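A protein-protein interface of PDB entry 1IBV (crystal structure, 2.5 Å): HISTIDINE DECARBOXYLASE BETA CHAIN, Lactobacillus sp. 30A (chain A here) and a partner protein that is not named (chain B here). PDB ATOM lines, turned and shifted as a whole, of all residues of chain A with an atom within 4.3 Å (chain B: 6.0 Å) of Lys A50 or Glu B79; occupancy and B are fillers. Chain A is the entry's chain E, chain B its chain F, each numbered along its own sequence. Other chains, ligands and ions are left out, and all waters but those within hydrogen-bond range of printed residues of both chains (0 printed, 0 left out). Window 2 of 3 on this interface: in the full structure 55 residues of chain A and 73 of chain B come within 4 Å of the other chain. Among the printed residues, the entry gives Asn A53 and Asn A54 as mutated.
Gln B171 touches Arg A48 (CG to O, 3.4 Å).
Asp A49 touches Gly B170 (CA to O, 3.8 Å).
CE of Lys A50 touches OE2 of Glu B79 (3.4 Å).
Asp A57 touches Ile B172 (CB to CG2, 3.9 Å).
Of chain B, only Glu B79 and Gly B170 come within 4 Å of Lys A50.
Glu B79 touches just one residue of chain A: Lys A50.
Of the printed residues of chain B, Arg A48 touches Gln B171 and Ile B172.
Printed residues of chain A within 4 Å of Ile B172: Arg A48 (2.8 Å) and Asp A57 (3.9 Å).
The nearest residue of chain B that does not touch Lys A50 is Gln B171 (4.1 Å).
Of the 16 printed residues of chain B, 4 touch a printed residue of chain A.
Printed residues of chain B that touch a printed residue of chain A: Glu B79, Gly B170, Gln B171 and Ile B172.
Hydrophobic or aromatic side chains of chain B within 4 Å of the printed part of chain A: Ile B172.
Among the printed residues, no Asp or Glu carboxylate lies within 4 Å of a Lys or Arg side-chain nitrogen of the other chain.
NE2 of Gln B171 lies within hydrogen-bond range of OD1 of Asp A49, at 2.9 Å.
The backbone carbonyl oxygen (O) of Arg A48 lies within hydrogen-bond range of the backbone NH (N) of Ile B172, at 2.8 Å.
The backbone NH (N) of Lys A50 lies within hydrogen-bond range of the backbone carbonyl oxygen (O) of Gly B170, 3.0 Å away.
N of Gly B92 sits at hydrogen-bond distance from O of Glu B79.
The backbone NH of Arg B80 sits at hydrogen-bond distance from the backbone carbonyl oxygen of Gln B171, at 3.0 Å.
N of Gly B170 is in hydrogen-bond range of O of Arg B80, at 2.7 Å.
The guanidinium group of Arg A48 lies within salt-bridge range of the side-chain carboxylate of Asp A57, at 2.9 Å.
OD1 of Asp A57 lies within hydrogen-bond range of OG of Ser A51.
The side-chain amino group (NZ) of Lys A50 lies within salt-bridge range of the side-chain carboxylate (OD2) of Asp A57 (3.1 Å).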
ATOM      1  N   ARG A  48     -10.446   7.430  14.802  1.00  0.00           N
ATOM      2  CA  ARG A  48     -11.895   7.619  14.774  1.00  0.00           C
ATOM      3  C   ARG A  48     -12.190   9.110  14.586  1.00  0.00           C
ATOM      4  O   ARG A  48     -11.466   9.965  15.111  1.00  0.00           O
ATOM      5  CB  ARG A  48     -12.538   7.110  16.067  1.00  0.00           C
ATOM      6  CG  ARG A  48     -13.677   7.989  16.598  1.00  0.00           C
ATOM      7  CD  ARG A  48     -14.996   7.240  16.733  1.00  0.00           C
ATOM      8  NE  ARG A  48     -15.665   7.616  17.972  1.00  0.00           N
ATOM      9  CZ  ARG A  48     -16.980   7.592  18.172  1.00  0.00           C
ATOM     10  NH1 ARG A  48     -17.807   7.203  17.211  1.00  0.00           N
ATOM     11  NH2 ARG A  48     -17.466   7.996  19.340  1.00  0.00           N
ATOM     12  N   ASP A  49     -13.237   9.422  13.829  1.00  0.00           N
ATOM     13  CA  ASP A  49     -13.603  10.819  13.600  1.00  0.00           C
ATOM     14  C   ASP A  49     -14.087  11.366  14.929  1.00  0.00           C
ATOM     15  O   ASP A  49     -14.878  10.717  15.619  1.00  0.00           O
ATOM     16  CB  ASP A  49     -14.692  10.924  12.533  1.00  0.00           C
ATOM     17  CG  ASP A  49     -14.248  10.354  11.192  1.00  0.00           C
ATOM     18  OD1 ASP A  49     -13.034  10.385  10.890  1.00  0.00           O
ATOM     19  OD2 ASP A  49     -15.112   9.859  10.438  1.00  0.00           O
ATOM     20  N   LYS A  50     -13.586  12.538  15.302  1.00  0.00           N
ATOM     21  CA  LYS A  50     -13.944  13.144  16.577  1.00  0.00           C
ATOM     22  C   LYS A  50     -15.428  13.371  16.764  1.00  0.00           C
ATOM     23  O   LYS A  50     -16.142  13.703  15.821  1.00  0.00           O
ATOM     24  CB  LYS A  50     -13.210  14.468  16.783  1.00  0.00           C
ATOM     25  CG  LYS A  50     -13.300  15.009  18.214  1.00  0.00           C
ATOM     26  CD  LYS A  50     -12.600  14.053  19.203  1.00  0.00           C
ATOM     27  CE  LYS A  50     -12.476  14.636  20.625  1.00  0.00           C
ATOM     28  NZ  LYS A  50     -13.779  14.774  21.349  1.00  0.00           N
ATOM     29  N   SER A  51     -15.886  13.127  17.983  1.00  0.00           N
ATOM     30  CA  SER A  51     -17.275  13.333  18.360  1.00  0.00           C
ATOM     31  C   SER A  51     -17.168  14.195  19.605  1.00  0.00           C
ATOM     32  O   SER A  51     -16.061  14.520  20.037  1.00  0.00           O
ATOM     33  CB  SER A  51     -17.934  12.001  18.722  1.00  0.00           C
ATOM     34  OG  SER A  51     -17.386  11.478  19.927  1.00  0.00           O
ATOM     35  N   ASN A  53     -17.603  13.238  22.437  1.00  0.00           N
ATOM     36  CA  ASN A  53     -17.392  12.303  23.538  1.00  0.00           C
ATOM     37  C   ASN A  53     -15.955  11.831  23.597  1.00  0.00           C
ATOM     38  O   ASN A  53     -15.568  10.899  22.888  1.00  0.00           O
ATOM     39  CB  ASN A  53     -18.304  11.085  23.389  1.00  0.00           C
ATOM     40  CG  ASN A  53     -19.502  11.360  22.501  1.00  0.00           C
ATOM     41  OD1 ASN A  53     -20.270  12.281  22.758  1.00  0.00           O
ATOM     42  ND2 ASN A  53     -19.639  10.596  21.417  1.00  0.00           N
ATOM     43  N   ASN A  54     -15.169  12.451  24.465  1.00  0.00           N
ATOM     44  CA  ASN A  54     -13.778  12.052  24.608  1.00  0.00           C
ATOM     45  C   ASN A  54     -13.684  10.563  24.940  1.00  0.00           C
ATOM     46  O   ASN A  54     -12.954   9.817  24.275  1.00  0.00           O
ATOM     47  CB  ASN A  54     -13.087  12.894  25.684  1.00  0.00           C
ATOM     48  CG  ASN A  54     -12.711  14.277  25.180  1.00  0.00           C
ATOM     49  OD1 ASN A  54     -11.659  14.454  24.542  1.00  0.00           O
ATOM     50  ND2 ASN A  54     -13.578  15.262  25.433  1.00  0.00           N
ATOM     51  N   ASP A  57     -14.670   8.229  22.013  1.00  0.00           N
ATOM     52  CA  ASP A  57     -13.669   8.329  20.964  1.00  0.00           C
ATOM     53  C   ASP A  57     -12.468   7.480  21.333  1.00  0.00           C
ATOM     54  O   ASP A  57     -11.861   6.847  20.463  1.00  0.00           O
ATOM     55  CB  ASP A  57     -13.252   9.779  20.757  1.00  0.00           C
ATOM     56  CG  ASP A  57     -14.369  10.616  20.173  1.00  0.00           C
ATOM     57  OD1 ASP A  57     -15.195  10.061  19.407  1.00  0.00           O
ATOM     58  OD2 ASP A  57     -14.429  11.827  20.488  1.00  0.00           O
ATOM     59  N   THR B  77      -3.541   8.944  23.714  1.00  0.00           N
ATOM     60  CA  THR B  77      -4.619   9.466  22.898  1.00  0.00           C
ATOM     61  C   THR B  77      -4.332  10.921  22.571  1.00  0.00           C
ATOM     62  O   THR B  77      -3.817  11.657  23.409  1.00  0.00           O
ATOM     63  CB  THR B  77      -5.950   9.315  23.659  1.00  0.00           C
ATOM     64  OG1 THR B  77      -6.431   7.980  23.486  1.00  0.00           O
ATOM     65  CG2 THR B  77      -7.004  10.314  23.188  1.00  0.00           C
ATOM     66  N   ALA B  78      -4.625  11.319  21.341  1.00  0.00           N
ATOM     67  CA  ALA B  78      -4.398  12.695  20.916  1.00  0.00           C
ATOM     68  C   ALA B  78      -5.373  13.075  19.820  1.00  0.00           C
ATOM     69  O   ALA B  78      -5.776  12.239  19.006  1.00  0.00           O
ATOM     70  CB  ALA B  78      -2.973  12.879  20.434  1.00  0.00           C
ATOM     71  N   GLU B  79      -5.730  14.349  19.785  1.00  0.00           N
ATOM     72  CA  GLU B  79      -6.669  14.842  18.794  1.00  0.00           C
ATOM     73  C   GLU B  79      -6.002  15.767  17.793  1.00  0.00           C
ATOM     74  O   GLU B  79      -4.984  16.406  18.095  1.00  0.00           O
ATOM     75  CB  GLU B  79      -7.788  15.606  19.502  1.00  0.00           C
ATOM     76  CG  GLU B  79      -8.810  16.233  18.562  1.00  0.00           C
ATOM     77  CD  GLU B  79      -9.796  17.128  19.281  1.00  0.00           C
ATOM     78  OE1 GLU B  79     -10.374  18.022  18.623  1.00  0.00           O
ATOM     79  OE2 GLU B  79      -9.993  16.941  20.505  1.00  0.00           O
ATOM     80  N   ARG B  80      -6.578  15.831  16.597  1.00  0.00           N
ATOM     81  CA  ARG B  80      -6.086  16.728  15.562  1.00  0.00           C
ATOM     82  C   ARG B  80      -7.318  17.478  15.054  1.00  0.00           C
ATOM     83  O   ARG B  80      -8.214  16.880  14.445  1.00  0.00           O
ATOM     84  CB  ARG B  80      -5.436  15.955  14.425  1.00  0.00           C
ATOM     85  CG  ARG B  80      -4.670  16.869  13.501  1.00  0.00           C
ATOM     86  CD  ARG B  80      -4.946  16.547  12.051  1.00  0.00           C
ATOM     87  NE  ARG B  80      -4.144  17.380  11.168  1.00  0.00           N
ATOM     88  CZ  ARG B  80      -3.940  17.112   9.884  1.00  0.00           C
ATOM     89  NH1 ARG B  80      -4.481  16.033   9.334  1.00  0.00           N
ATOM     90  NH2 ARG B  80      -3.165  17.910   9.159  1.00  0.00           N
ATOM     91  N   PRO B  81      -7.397  18.799  15.306  1.00  0.00           N
ATOM     92  CA  PRO B  81      -8.541  19.609  14.868  1.00  0.00           C
ATOM     93  C   PRO B  81      -8.746  19.632  13.365  1.00  0.00           C
ATOM     94  O   PRO B  81      -7.972  19.040  12.605  1.00  0.00           O
ATOM     95  CB  PRO B  81      -8.182  21.010  15.377  1.00  0.00           C
ATOM     96  CG  PRO B  81      -7.304  20.736  16.561  1.00  0.00           C
ATOM     97  CD  PRO B  81      -6.426  19.626  16.042  1.00  0.00           C
ATOM     98  N   MET B  87      -3.901  24.596  18.359  1.00  0.00           N
ATOM     99  CA  MET B  87      -4.074  23.172  18.634  1.00  0.00           C
ATOM    100  C   MET B  87      -4.229  22.832  20.111  1.00  0.00           C
ATOM    101  O   MET B  87      -4.107  21.663  20.503  1.00  0.00           O
ATOM    102  CB  MET B  87      -2.921  22.354  18.035  1.00  0.00           C
ATOM    103  CG  MET B  87      -2.982  22.180  16.526  1.00  0.00           C
ATOM    104  SD  MET B  87      -2.157  20.635  16.017  1.00  0.00           S
ATOM    105  CE  MET B  87      -0.441  20.942  16.627  1.00  0.00           C
ATOM    106  N   LYS B  88      -4.494  23.840  20.939  1.00  0.00           N
ATOM    107  CA  LYS B  88      -4.650  23.603  22.372  1.00  0.00           C
ATOM    108  C   LYS B  88      -3.415  22.893  22.947  1.00  0.00           C
ATOM    109  O   LYS B  88      -2.443  22.629  22.219  1.00  0.00           O
ATOM    110  CB  LYS B  88      -5.934  22.805  22.643  1.00  0.00           C
ATOM    111  CG  LYS B  88      -7.214  23.650  22.667  1.00  0.00           C
ATOM    112  CD  LYS B  88      -7.570  24.213  21.298  1.00  0.00           C
ATOM    113  CE  LYS B  88      -8.112  23.132  20.381  1.00  0.00           C
ATOM    114  NZ  LYS B  88      -8.590  23.695  19.076  1.00  0.00           N
ATOM    115  N   GLY B  90      -2.425  19.475  24.783  1.00  0.00           N
ATOM    116  CA  GLY B  90      -1.998  18.146  24.362  1.00  0.00           C
ATOM    117  C   GLY B  90      -2.450  17.532  23.046  1.00  0.00           C
ATOM    118  O   GLY B  90      -2.525  16.307  22.941  1.00  0.00           O
ATOM    119  N   GLN B  91      -2.716  18.342  22.032  1.00  0.00           N
ATOM    120  CA  GLN B  91      -3.165  17.787  20.758  1.00  0.00           C
ATOM    121  C   GLN B  91      -1.992  17.613  19.801  1.00  0.00           C
ATOM    122  O   GLN B  91      -0.861  17.976  20.134  1.00  0.00           O
ATOM    123  CB  GLN B  91      -4.269  18.658  20.151  1.00  0.00           C
ATOM    124  CG  GLN B  91      -5.444  18.864  21.101  1.00  0.00           C
ATOM    125  CD  GLN B  91      -6.591  19.653  20.485  1.00  0.00           C
ATOM    126  OE1 GLN B  91      -6.452  20.252  19.409  1.00  0.00           O
ATOM    127  NE2 GLN B  91      -7.740  19.653  21.164  1.00  0.00           N
ATOM    128  N   GLY B  92      -2.247  17.042  18.627  1.00  0.00           N
ATOM    129  CA  GLY B  92      -1.159  16.831  17.688  1.00  0.00           C
ATOM    130  C   GLY B  92      -1.569  16.306  16.321  1.00  0.00           C
ATOM    131  O   GLY B  92      -2.758  16.187  16.010  1.00  0.00           O
ATOM    132  N   TYR B  93      -0.566  15.981  15.509  1.00  0.00           N
ATOM    133  CA  TYR B  93      -0.789  15.480  14.157  1.00  0.00           C
ATOM    134  C   TYR B  93      -0.741  13.964  14.113  1.00  0.00           C
ATOM    135  O   TYR B  93      -1.538  13.324  13.423  1.00  0.00           O
ATOM    136  CB  TYR B  93       0.260  16.063  13.183  1.00  0.00           C
ATOM    137  CG  TYR B  93       0.072  17.540  12.855  1.00  0.00           C
ATOM    138  CD1 TYR B  93      -0.874  17.948  11.910  1.00  0.00           C
ATOM    139  CD2 TYR B  93       0.815  18.519  13.512  1.00  0.00           C
ATOM    140  CE1 TYR B  93      -1.081  19.290  11.631  1.00  0.00           C
ATOM    141  CE2 TYR B  93       0.618  19.863  13.248  1.00  0.00           C
ATOM    142  CZ  TYR B  93      -0.332  20.248  12.307  1.00  0.00           C
ATOM    143  OH  TYR B  93      -0.539  21.586  12.045  1.00  0.00           O
ATOM    144  N   MET B 167      -3.299  11.400  12.116  1.00  0.00           N
ATOM    145  CA  MET B 167      -4.707  11.742  11.997  1.00  0.00           C
ATOM    146  C   MET B 167      -5.071  12.715  10.897  1.00  0.00           C
ATOM    147  O   MET B 167      -4.295  13.615  10.544  1.00  0.00           O
ATOM    148  CB  MET B 167      -5.252  12.281  13.319  1.00  0.00           C
ATOM    149  CG  MET B 167      -5.200  11.308  14.463  1.00  0.00           C
ATOM    150  SD  MET B 167      -3.553  11.200  15.139  1.00  0.00           S
ATOM    151  CE  MET B 167      -3.724  12.317  16.540  1.00  0.00           C
ATOM    152  N   GLY B 170      -9.757  16.751  12.286  1.00  0.00           N
ATOM    153  CA  GLY B 170     -10.938  16.399  13.064  1.00  0.00           C
ATOM    154  C   GLY B 170     -11.012  14.911  13.370  1.00  0.00           C
ATOM    155  O   GLY B 170     -12.092  14.323  13.472  1.00  0.00           O
ATOM    156  N   GLN B 171      -9.854  14.296  13.539  1.00  0.00           N
ATOM    157  CA  GLN B 171      -9.789  12.880  13.822  1.00  0.00           C
ATOM    158  C   GLN B 171      -8.962  12.685  15.087  1.00  0.00           C
ATOM    159  O   GLN B 171      -8.084  13.500  15.416  1.00  0.00           O
ATOM    160  CB  GLN B 171      -9.129  12.169  12.646  1.00  0.00           C
ATOM    161  CG  GLN B 171      -9.466  10.723  12.527  1.00  0.00           C
ATOM    162  CD  GLN B 171      -9.147  10.186  11.151  1.00  0.00           C
ATOM    163  OE1 GLN B 171      -7.985  10.095  10.750  1.00  0.00           O
ATOM    164  NE2 GLN B 171     -10.185   9.830  10.416  1.00  0.00           N
ATOM    165  N   ILE B 172      -9.265  11.627  15.822  1.00  0.00           N
ATOM    166  CA  ILE B 172      -8.545  11.341  17.047  1.00  0.00           C
ATOM    167  C   ILE B 172      -7.826  10.021  16.837  1.00  0.00           C
ATOM    168  O   ILE B 172      -8.317   9.138  16.120  1.00  0.00           O
ATOM    169  CB  ILE B 172      -9.506  11.281  18.248  1.00  0.00           C
ATOM    170  CG1 ILE B 172      -8.724  11.052  19.541  1.00  0.00           C
ATOM    171  CG2 ILE B 172     -10.546  10.197  18.025  1.00  0.00           C
ATOM    172  CD1 ILE B 172      -9.560  11.191  20.814  1.00  0.00           C
ATOM    173  N   GLY B 173      -6.629   9.918  17.392  1.00  0.00           N
ATOM    174  CA  GLY B 173      -5.857   8.703  17.236  1.00  0.00           C
ATOM    175  C   GLY B 173      -5.502   8.066  18.563  1.00  0.00           C
ATOM    176  O   GLY B 173      -5.359   8.759  19.579  1.00  0.00           O
